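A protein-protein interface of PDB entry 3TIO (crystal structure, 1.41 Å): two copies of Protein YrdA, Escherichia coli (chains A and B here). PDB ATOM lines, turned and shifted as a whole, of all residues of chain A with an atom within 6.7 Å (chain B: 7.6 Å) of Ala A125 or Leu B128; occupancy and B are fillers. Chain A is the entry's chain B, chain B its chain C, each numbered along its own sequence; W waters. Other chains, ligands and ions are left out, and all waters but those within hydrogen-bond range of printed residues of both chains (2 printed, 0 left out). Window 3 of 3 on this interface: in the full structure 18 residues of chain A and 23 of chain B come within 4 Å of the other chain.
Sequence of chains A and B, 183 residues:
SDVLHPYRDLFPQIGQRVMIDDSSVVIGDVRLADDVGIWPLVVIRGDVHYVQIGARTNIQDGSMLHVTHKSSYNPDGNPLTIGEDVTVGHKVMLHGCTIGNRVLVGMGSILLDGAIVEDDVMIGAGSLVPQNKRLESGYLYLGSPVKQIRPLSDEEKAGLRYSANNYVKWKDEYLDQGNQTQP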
ATOM      1  N   LEU A 104       4.142  19.598   5.340  1.00  0.00           N
ATOM      2  CA  LEU A 104       5.039  19.367   4.222  1.00  0.00           C
ATOM      3  C   LEU A 104       6.095  20.458   4.267  1.00  0.00           C
ATOM      4  O   LEU A 104       5.778  21.640   4.183  1.00  0.00           O
ATOM      5  CB  LEU A 104       4.280  19.402   2.890  1.00  0.00           C
ATOM      6  CG  LEU A 104       5.115  19.082   1.644  1.00  0.00           C
ATOM      7  CD1 LEU A 104       4.202  18.619   0.516  1.00  0.00           C
ATOM      8  CD2 LEU A 104       5.922  20.303   1.228  1.00  0.00           C
ATOM      9  N   VAL A 105       7.351  20.054   4.438  1.00  0.00           N
ATOM     10  CA  VAL A 105       8.461  21.000   4.485  1.00  0.00           C
ATOM     11  C   VAL A 105       9.138  20.976   3.116  1.00  0.00           C
ATOM     12  O   VAL A 105       9.803  20.002   2.752  1.00  0.00           O
ATOM     13  CB  VAL A 105       9.484  20.618   5.581  1.00  0.00           C
ATOM     14  CG1 VAL A 105      10.514  21.734   5.744  1.00  0.00           C
ATOM     15  CG2 VAL A 105       8.764  20.364   6.900  1.00  0.00           C
ATOM     16  N   GLY A 106       8.944  22.057   2.363  1.00  0.00           N
ATOM     17  CA  GLY A 106       9.504  22.166   1.027  1.00  0.00           C
ATOM     18  C   GLY A 106      10.992  21.904   0.945  1.00  0.00           C
ATOM     19  O   GLY A 106      11.758  22.363   1.794  1.00  0.00           O
ATOM     20  N   MET A 107      11.402  21.184  -0.095  1.00  0.00           N
ATOM     21  CA  MET A 107      12.806  20.842  -0.282  1.00  0.00           C
ATOM     22  C   MET A 107      13.733  22.043  -0.181  1.00  0.00           C
ATOM     23  O   MET A 107      13.412  23.143  -0.639  1.00  0.00           O
ATOM     24  CB  MET A 107      13.008  20.126  -1.628  1.00  0.00           C
ATOM     25  CG  MET A 107      12.732  20.966  -2.860  1.00  0.00           C
ATOM     26  SD  MET A 107      12.779  19.948  -4.364  1.00  0.00           S
ATOM     27  CE  MET A 107      11.058  19.564  -4.557  1.00  0.00           C
ATOM     28  N   GLY A 108      14.885  21.823   0.445  1.00  0.00           N
ATOM     29  CA  GLY A 108      15.878  22.867   0.599  1.00  0.00           C
ATOM     30  C   GLY A 108      15.610  23.881   1.693  1.00  0.00           C
ATOM     31  O   GLY A 108      16.355  24.850   1.823  1.00  0.00           O
ATOM     32  N   SER A 109      14.565  23.669   2.482  1.00  0.00           N
ATOM     33  CA  SER A 109      14.235  24.603   3.555  1.00  0.00           C
ATOM     34  C   SER A 109      15.092  24.407   4.799  1.00  0.00           C
ATOM     35  O   SER A 109      15.690  23.348   5.004  1.00  0.00           O
ATOM     36  CB  SER A 109      12.758  24.474   3.943  1.00  0.00           C
ATOM     37  OG  SER A 109      11.911  24.893   2.887  1.00  0.00           O
ATOM     38  N   ILE A 123       5.224  24.438   3.826  1.00  0.00           N
ATOM     39  CA  ILE A 123       6.328  25.386   3.759  1.00  0.00           C
ATOM     40  C   ILE A 123       6.923  25.252   2.361  1.00  0.00           C
ATOM     41  O   ILE A 123       7.308  24.161   1.944  1.00  0.00           O
ATOM     42  CB  ILE A 123       7.399  25.065   4.827  1.00  0.00           C
ATOM     43  CG1 ILE A 123       6.805  25.252   6.226  1.00  0.00           C
ATOM     44  CG2 ILE A 123       8.608  25.969   4.641  1.00  0.00           C
ATOM     45  CD1 ILE A 123       7.686  24.737   7.350  1.00  0.00           C
ATOM     46  N   GLY A 124       6.970  26.359   1.630  1.00  0.00           N
ATOM     47  CA  GLY A 124       7.498  26.323   0.278  1.00  0.00           C
ATOM     48  C   GLY A 124       8.968  25.962   0.215  1.00  0.00           C
ATOM     49  O   GLY A 124       9.708  26.165   1.177  1.00  0.00           O
ATOM     50  N   ALA A 125       9.396  25.429  -0.924  1.00  0.00           N
ATOM     51  CA  ALA A 125      10.794  25.051  -1.101  1.00  0.00           C
ATOM     52  C   ALA A 125      11.718  26.245  -0.881  1.00  0.00           C
ATOM     53  O   ALA A 125      11.359  27.386  -1.171  1.00  0.00           O
ATOM     54  CB  ALA A 125      11.006  24.486  -2.502  1.00  0.00           C
ATOM     55  N   GLY A 126      12.909  25.972  -0.353  1.00  0.00           N
ATOM     56  CA  GLY A 126      13.895  27.017  -0.130  1.00  0.00           C
ATOM     57  C   GLY A 126      13.582  28.079   0.904  1.00  0.00           C
ATOM     58  O   GLY A 126      14.156  29.166   0.861  1.00  0.00           O
ATOM     59  N   SER A 127      12.693  27.769   1.841  1.00  0.00           N
ATOM     60  CA  SER A 127      12.314  28.720   2.877  1.00  0.00           C
ATOM     61  C   SER A 127      13.196  28.606   4.106  1.00  0.00           C
ATOM     62  O   SER A 127      13.895  27.612   4.295  1.00  0.00           O
ATOM     63  CB  SER A 127      10.864  28.491   3.305  1.00  0.00           C
ATOM     64  OG  SER A 127       9.965  28.696   2.229  1.00  0.00           O
ATOM     65  N   TYR A 141       3.328  28.833   3.981  1.00  0.00           N
ATOM     66  CA  TYR A 141       4.376  29.775   4.352  1.00  0.00           C
ATOM     67  C   TYR A 141       5.502  29.640   3.346  1.00  0.00           C
ATOM     68  O   TYR A 141       5.811  28.538   2.908  1.00  0.00           O
ATOM     69  CB  TYR A 141       4.932  29.463   5.744  1.00  0.00           C
ATOM     70  CG  TYR A 141       4.016  29.821   6.883  1.00  0.00           C
ATOM     71  CD1 TYR A 141       2.962  28.985   7.249  1.00  0.00           C
ATOM     72  CD2 TYR A 141       4.200  31.005   7.593  1.00  0.00           C
ATOM     73  CE1 TYR A 141       2.111  29.325   8.302  1.00  0.00           C
ATOM     74  CE2 TYR A 141       3.359  31.354   8.641  1.00  0.00           C
ATOM     75  CZ  TYR A 141       2.318  30.511   8.992  1.00  0.00           C
ATOM     76  OH  TYR A 141       1.490  30.859  10.037  1.00  0.00           O
ATOM     77  N   LEU A 142       6.117  30.754   2.975  1.00  0.00           N
ATOM     78  CA  LEU A 142       7.221  30.693   2.032  1.00  0.00           C
ATOM     79  C   LEU A 142       8.099  31.926   2.127  1.00  0.00           C
ATOM     80  O   LEU A 142       7.635  33.007   2.498  1.00  0.00           O
ATOM     81  CB  LEU A 142       6.693  30.518   0.602  1.00  0.00           C
ATOM     82  CG  LEU A 142       5.825  31.622  -0.001  1.00  0.00           C
ATOM     83  CD1 LEU A 142       6.704  32.767  -0.487  1.00  0.00           C
ATOM     84  CD2 LEU A 142       5.022  31.052  -1.163  1.00  0.00           C
ATOM     85  N   GLY A 143       9.375  31.745   1.805  1.00  0.00           N
ATOM     86  CA  GLY A 143      10.317  32.844   1.849  1.00  0.00           C
ATOM     87  C   GLY A 143      11.441  32.650   2.847  1.00  0.00           C
ATOM     88  O   GLY A 143      11.416  31.730   3.665  1.00  0.00           O
ATOM     89  N   MET B  93      20.124  21.363  -6.210  1.00  0.00           N
ATOM     90  CA  MET B  93      18.923  20.544  -6.101  1.00  0.00           C
ATOM     91  C   MET B  93      18.150  20.681  -7.414  1.00  0.00           C
ATOM     92  O   MET B  93      17.694  21.773  -7.748  1.00  0.00           O
ATOM     93  CB  MET B  93      18.074  21.064  -4.935  1.00  0.00           C
ATOM     94  CG  MET B  93      16.710  20.423  -4.772  1.00  0.00           C
ATOM     95  SD  MET B  93      16.709  18.879  -3.852  1.00  0.00           S
ATOM     96  CE  MET B  93      15.991  17.778  -5.068  1.00  0.00           C
ATOM     97  N   GLY B 108      24.522  25.533  -4.948  1.00  0.00           N
ATOM     98  CA  GLY B 108      23.506  25.787  -3.942  1.00  0.00           C
ATOM     99  C   GLY B 108      22.130  26.151  -4.469  1.00  0.00           C
ATOM    100  O   GLY B 108      21.217  26.405  -3.685  1.00  0.00           O
ATOM    101  N   SER B 109      21.959  26.169  -5.786  1.00  0.00           N
ATOM    102  CA  SER B 109      20.663  26.520  -6.358  1.00  0.00           C
ATOM    103  C   SER B 109      19.629  25.404  -6.259  1.00  0.00           C
ATOM    104  O   SER B 109      19.970  24.235  -6.041  1.00  0.00           O
ATOM    105  CB  SER B 109      20.828  26.936  -7.821  1.00  0.00           C
ATOM    106  OG  SER B 109      21.597  28.123  -7.927  1.00  0.00           O
ATOM    107  N   ILE B 110      18.364  25.785  -6.422  1.00  0.00           N
ATOM    108  CA  ILE B 110      17.236  24.862  -6.375  1.00  0.00           C
ATOM    109  C   ILE B 110      16.365  25.105  -7.601  1.00  0.00           C
ATOM    110  O   ILE B 110      15.855  26.210  -7.789  1.00  0.00           O
ATOM    111  CB  ILE B 110      16.363  25.091  -5.104  1.00  0.00           C
ATOM    112  CG1 ILE B 110      17.201  24.868  -3.841  1.00  0.00           C
ATOM    113  CG2 ILE B 110      15.157  24.156  -5.118  1.00  0.00           C
ATOM    114  CD1 ILE B 110      16.478  25.234  -2.553  1.00  0.00           C
ATOM    115  N   LEU B 111      16.219  24.082  -8.440  1.00  0.00           N
ATOM    116  CA  LEU B 111      15.386  24.171  -9.640  1.00  0.00           C
ATOM    117  C   LEU B 111      14.198  23.242  -9.438  1.00  0.00           C
ATOM    118  O   LEU B 111      14.356  22.025  -9.311  1.00  0.00           O
ATOM    119  CB  LEU B 111      16.181  23.783 -10.895  1.00  0.00           C
ATOM    120  CG  LEU B 111      17.010  24.915 -11.520  1.00  0.00           C
ATOM    121  CD1 LEU B 111      18.028  25.439 -10.526  1.00  0.00           C
ATOM    122  CD2 LEU B 111      17.699  24.405 -12.786  1.00  0.00           C
ATOM    123  N   LEU B 112      13.005  23.823  -9.409  1.00  0.00           N
ATOM    124  CA  LEU B 112      11.792  23.065  -9.155  1.00  0.00           C
ATOM    125  C   LEU B 112      11.083  22.452 -10.353  1.00  0.00           C
ATOM    126  O   LEU B 112      11.447  22.680 -11.506  1.00  0.00           O
ATOM    127  CB  LEU B 112      10.823  23.928  -8.342  1.00  0.00           C
ATOM    128  CG  LEU B 112      11.410  24.433  -7.016  1.00  0.00           C
ATOM    129  CD1 LEU B 112      10.421  25.363  -6.340  1.00  0.00           C
ATOM    130  CD2 LEU B 112      11.750  23.252  -6.111  1.00  0.00           C
ATOM    131  N   ASP B 113      10.063  21.661 -10.041  1.00  0.00           N
ATOM    132  CA  ASP B 113       9.278  20.929 -11.023  1.00  0.00           C
ATOM    133  C   ASP B 113       8.731  21.745 -12.183  1.00  0.00           C
ATOM    134  O   ASP B 113       8.146  22.809 -11.992  1.00  0.00           O
ATOM    135  CB  ASP B 113       8.131  20.225 -10.303  1.00  0.00           C
ATOM    136  CG  ASP B 113       8.621  19.336  -9.179  1.00  0.00           C
ATOM    137  OD1 ASP B 113       8.841  18.131  -9.419  1.00  0.00           O
ATOM    138  OD2 ASP B 113       8.808  19.852  -8.058  1.00  0.00           O
ATOM    139  N   ILE B 123      22.911  30.538 -14.144  1.00  0.00           N
ATOM    140  CA  ILE B 123      22.093  30.767 -12.960  1.00  0.00           C
ATOM    141  C   ILE B 123      23.062  31.017 -11.812  1.00  0.00           C
ATOM    142  O   ILE B 123      23.935  30.198 -11.539  1.00  0.00           O
ATOM    143  CB  ILE B 123      21.210  29.538 -12.646  1.00  0.00           C
ATOM    144  CG1 ILE B 123      20.211  29.313 -13.787  1.00  0.00           C
ATOM    145  CG2 ILE B 123      20.479  29.744 -11.322  1.00  0.00           C
ATOM    146  CD1 ILE B 123      19.469  27.990 -13.708  1.00  0.00           C
ATOM    147  N   GLY B 124      22.921  32.157 -11.147  1.00  0.00           N
ATOM    148  CA  GLY B 124      23.821  32.466 -10.053  1.00  0.00           C
ATOM    149  C   GLY B 124      23.684  31.539  -8.862  1.00  0.00           C
ATOM    150  O   GLY B 124      22.638  30.925  -8.654  1.00  0.00           O
ATOM    151  N   ALA B 125      24.746  31.448  -8.072  1.00  0.00           N
ATOM    152  CA  ALA B 125      24.742  30.603  -6.885  1.00  0.00           C
ATOM    153  C   ALA B 125      23.623  30.992  -5.917  1.00  0.00           C
ATOM    154  O   ALA B 125      23.252  32.161  -5.812  1.00  0.00           O
ATOM    155  CB  ALA B 125      26.093  30.699  -6.181  1.00  0.00           C
ATOM    156  N   GLY B 126      23.087  29.993  -5.220  1.00  0.00           N
ATOM    157  CA  GLY B 126      22.036  30.226  -4.244  1.00  0.00           C
ATOM    158  C   GLY B 126      20.709  30.702  -4.794  1.00  0.00           C
ATOM    159  O   GLY B 126      19.917  31.309  -4.068  1.00  0.00           O
ATOM    160  N   SER B 127      20.452  30.422  -6.067  1.00  0.00           N
ATOM    161  CA  SER B 127      19.200  30.837  -6.691  1.00  0.00           C
ATOM    162  C   SER B 127      18.098  29.796  -6.548  1.00  0.00           C
ATOM    163  O   SER B 127      18.351  28.625  -6.258  1.00  0.00           O
ATOM    164  CB  SER B 127      19.411  31.111  -8.182  1.00  0.00           C
ATOM    165  OG  SER B 127      20.304  32.189  -8.391  1.00  0.00           O
ATOM    166  N   LEU B 128      16.864  30.238  -6.753  1.00  0.00           N
ATOM    167  CA  LEU B 128      15.726  29.339  -6.702  1.00  0.00           C
ATOM    168  C   LEU B 128      14.867  29.600  -7.932  1.00  0.00           C
ATOM    169  O   LEU B 128      14.419  30.725  -8.163  1.00  0.00           O
ATOM    170  CB  LEU B 128      14.909  29.550  -5.421  1.00  0.00           C
ATOM    171  CG  LEU B 128      13.753  28.556  -5.240  1.00  0.00           C
ATOM    172  CD1 LEU B 128      13.399  28.420  -3.766  1.00  0.00           C
ATOM    173  CD2 LEU B 128      12.552  29.011  -6.053  1.00  0.00           C
ATOM    174  N   VAL B 129      14.672  28.562  -8.738  1.00  0.00           N
ATOM    175  CA  VAL B 129      13.853  28.663  -9.939  1.00  0.00           C
ATOM    176  C   VAL B 129      12.505  28.027  -9.622  1.00  0.00           C
ATOM    177  O   VAL B 129      12.418  26.820  -9.395  1.00  0.00           O
ATOM    178  CB  VAL B 129      14.505  27.920 -11.123  1.00  0.00           C
ATOM    179  CG1 VAL B 129      13.644  28.067 -12.366  1.00  0.00           C
ATOM    180  CG2 VAL B 129      15.902  28.468 -11.371  1.00  0.00           C
ATOM    181  N   PRO B 130      11.433  28.836  -9.595  1.00  0.00           N
ATOM    182  CA  PRO B 130      10.072  28.380  -9.298  1.00  0.00           C
ATOM    183  C   PRO B 130       9.543  27.325 -10.255  1.00  0.00           C
ATOM    184  O   PRO B 130      10.035  27.179 -11.372  1.00  0.00           O
ATOM    185  CB  PRO B 130       9.247  29.664  -9.372  1.00  0.00           C
ATOM    186  CG  PRO B 130      10.231  30.732  -9.042  1.00  0.00           C
ATOM    187  CD  PRO B 130      11.453  30.293  -9.810  1.00  0.00           C
ATOM    188  N   GLN B 131       8.521  26.604  -9.809  1.00  0.00           N
ATOM    189  CA  GLN B 131       7.910  25.570 -10.628  1.00  0.00           C
ATOM    190  C   GLN B 131       7.421  26.154 -11.952  1.00  0.00           C
ATOM    191  O   GLN B 131       6.888  27.266 -11.994  1.00  0.00           O
ATOM    192  CB  GLN B 131       6.719  24.937  -9.899  1.00  0.00           C
ATOM    193  CG  GLN B 131       7.026  24.397  -8.514  1.00  0.00           C
ATOM    194  CD  GLN B 131       5.824  23.720  -7.877  1.00  0.00           C
ATOM    195  OE1 GLN B 131       4.735  24.293  -7.815  1.00  0.00           O
ATOM    196  NE2 GLN B 131       6.017  22.498  -7.398  1.00  0.00           N
ATOM    197  N   LYS B 133       8.728  27.663 -14.322  1.00  0.00           N
ATOM    198  CA  LYS B 133       9.316  28.872 -14.880  1.00  0.00           C
ATOM    199  C   LYS B 133      10.260  28.562 -16.036  1.00  0.00           C
ATOM    200  O   LYS B 133      11.073  27.637 -15.966  1.00  0.00           O
ATOM    201  CB  LYS B 133      10.069  29.660 -13.806  1.00  0.00           C
ATOM    202  CG  LYS B 133      10.603  30.991 -14.320  1.00  0.00           C
ATOM    203  CD  LYS B 133      11.304  31.792 -13.240  1.00  0.00           C
ATOM    204  CE  LYS B 133      11.734  33.152 -13.771  1.00  0.00           C
ATOM    205  NZ  LYS B 133      10.576  33.958 -14.253  1.00  0.00           N
ATOM    206  N   LEU B 135      13.336  29.766 -18.370  1.00  0.00           N
ATOM    207  CA  LEU B 135      14.462  30.688 -18.396  1.00  0.00           C
ATOM    208  C   LEU B 135      14.939  30.814 -19.839  1.00  0.00           C
ATOM    209  O   LEU B 135      15.478  29.868 -20.414  1.00  0.00           O
ATOM    210  CB  LEU B 135      15.604  30.184 -17.508  1.00  0.00           C
ATOM    211  CG  LEU B 135      15.294  29.916 -16.029  1.00  0.00           C
ATOM    212  CD1 LEU B 135      16.612  29.773 -15.273  1.00  0.00           C
ATOM    213  CD2 LEU B 135      14.465  31.042 -15.438  1.00  0.00           C
ATOM    214  N   LEU B 142      19.405  35.349 -11.595  1.00  0.00           N
ATOM    215  CA  LEU B 142      19.902  35.380 -10.224  1.00  0.00           C
ATOM    216  C   LEU B 142      18.776  35.690  -9.258  1.00  0.00           C
ATOM    217  O   LEU B 142      17.853  36.425  -9.599  1.00  0.00           O
ATOM    218  CB  LEU B 142      20.963  36.474 -10.070  1.00  0.00           C
ATOM    219  CG  LEU B 142      22.395  36.260 -10.553  1.00  0.00           C
ATOM    220  CD1 LEU B 142      23.059  37.604 -10.800  1.00  0.00           C
ATOM    221  CD2 LEU B 142      23.162  35.472  -9.508  1.00  0.00           C
ATOM    222  N   GLY B 143      18.860  35.131  -8.055  1.00  0.00           N
ATOM    223  CA  GLY B 143      17.854  35.414  -7.050  1.00  0.00           C
ATOM    224  C   GLY B 143      16.991  34.264  -6.583  1.00  0.00           C
ATOM    225  O   GLY B 143      17.002  33.174  -7.156  1.00  0.00           O
ATOM    226  N   SER B 144      16.239  34.528  -5.519  1.00  0.00           N
ATOM    227  CA  SER B 144      15.333  33.555  -4.930  1.00  0.00           C
ATOM    228  C   SER B 144      14.001  34.243  -4.651  1.00  0.00           C
ATOM    229  O   SER B 144      13.826  34.863  -3.605  1.00  0.00           O
ATOM    230  CB  SER B 144      15.914  33.016  -3.621  1.00  0.00           C
ATOM    231  OG  SER B 144      15.027  32.091  -3.020  1.00  0.00           O
ATOM    232  N   PRO B 145      13.045  34.152  -5.589  1.00  0.00           N
ATOM    233  CA  PRO B 145      13.138  33.453  -6.874  1.00  0.00           C
ATOM    234  C   PRO B 145      13.962  34.231  -7.893  1.00  0.00           C
ATOM    235  O   PRO B 145      14.137  35.443  -7.770  1.00  0.00           O
ATOM    236  CB  PRO B 145      11.680  33.317  -7.287  1.00  0.00           C
ATOM    237  CG  PRO B 145      11.097  34.595  -6.792  1.00  0.00           C
ATOM    238  CD  PRO B 145      11.703  34.734  -5.411  1.00  0.00           C
ATOM    239  N   VAL B 146      14.464  33.532  -8.905  1.00  0.00           N
ATOM    240  CA  VAL B 146      15.285  34.177  -9.917  1.00  0.00           C
ATOM    241  C   VAL B 146      14.575  35.250 -10.724  1.00  0.00           C
ATOM    242  O   VAL B 146      13.356  35.223 -10.922  1.00  0.00           O
ATOM    243  CB  VAL B 146      15.867  33.163 -10.939  1.00  0.00           C
ATOM    244  CG1 VAL B 146      16.788  32.181 -10.241  1.00  0.00           C
ATOM    245  CG2 VAL B 146      14.742  32.444 -11.665  1.00  0.00           C
ATOM    246  N   LYS B 147      15.378  36.197 -11.187  1.00  0.00           N
ATOM    247  CA  LYS B 147      14.922  37.284 -12.029  1.00  0.00           C
ATOM    248  C   LYS B 147      15.868  37.280 -13.220  1.00  0.00           C
ATOM    249  O   LYS B 147      17.032  36.897 -13.089  1.00  0.00           O
ATOM    250  CB  LYS B 147      15.027  38.626 -11.300  1.00  0.00           C
ATOM    251  CG  LYS B 147      14.038  38.810 -10.161  1.00  0.00           C
ATOM    252  CD  LYS B 147      14.196  40.191  -9.541  1.00  0.00           C
ATOM    253  CE  LYS B 147      13.160  40.446  -8.461  1.00  0.00           C
ATOM    254  NZ  LYS B 147      13.327  41.798  -7.857  1.00  0.00           N
HETATM  255  O   HOH W   1      15.863  30.482  -0.878  1.00  0.00           O
HETATM  256  O   HOH W   2      13.313  32.007  -0.691  1.00  0.00           O
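O of Leu B128 lies within hydrogen-bond range of N of Val B146. The backbone carbonyl oxygen of Met A107 lies within hydrogen-bond range of the backbone NH of Gly A126, at 2.9 Å. O of Met B93 is in hydrogen-bond range of N of Leu B111 (2.8 Å). The backbone carbonyl oxygen (O) of Val B129 is in hydrogen-bond range of the backbone NH (N) of Leu B112, at 3.1 Å. The backbone NH of Ile B110 is in hydrogen-bond range of the backbone carbonyl oxygen of Ser B127 (2.8 Å). The backbone NH (N) of Met B93 lies within hydrogen-bond range of the backbone carbonyl oxygen (O) of Ser B109 (2.9 Å).
Among the printed residues, merely in contact across the chains: Ala A125 with Leu B128 (3.5 Å), Met A107 with Leu B112 (3.9 Å), Ala A125 with Leu B112 (3.9 Å), Gly A126 with Leu B128 (3.9 Å), Met A107 with Met B93 (3.9 Å), Gly A126 with Ile B110 (3.97 Å) and Gly A108 with Ile B110 (3.99 Å).
Of the printed residues of chain B, Met A107 touches Met B93 and Leu B112. Printed residues of chain B within 4 Å of Gly A108: Ile B110. Ala A125 touches two residues of chain B. Of the printed residues of chain B, Gly A126 touches Ile B110 (3.97 Å) and Leu B128 (3.9 Å). Printed residues of chain A within 4 Å of Ile B110: Gly A108 (3.99 Å) and Gly A126 (3.97 Å). Leu B128 touches just these residues of chain A: Ala A125 (3.5 Å) and Gly A126 (3.9 Å). The nearest residue of chain B that does not touch Ala A125 is Ile B110 (4.9 Å). The nearest residue of chain A that does not touch Leu B128 is Ser A127 (5.7 Å). The nearest printed residue of chain B that does not touch Gly A108 is Met B93 (5.5 Å).
Of the 24 printed residues of chain B, 4 touch a printed residue of chain A. Hydrophobic or aromatic side chains of chain B that line the printed part of chain A: Met B93, Ile B110, Leu B112 and Leu B128. Printed residues of chain A that touch a printed residue of chain B: Met A107, Gly A108, Ala A125 and Gly A126. Along chain A the printed residues that touch a printed residue of chain B span positions 107 to 126. Among the printed residues, no Asp or Glu carboxylate lies within 4 Å of a Lys or Arg side-chain nitrogen of the other chain.
Positions printed for both chains: 108, 109, 123, 124, 125, 126, 127, 142 and 143. Of the 7 pairs that touch across the chains among the printed residues, none has its exchanged pair printed and touching as well.
Water W1 bridges O of Gly A126 and OG of Ser B144. Water W2 lies within hydrogen-bond range of the side-chain hydroxyl of Ser B144 (2.9 Å) and the backbone carbonyl oxygen of Gly A126 (3.3 Å).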
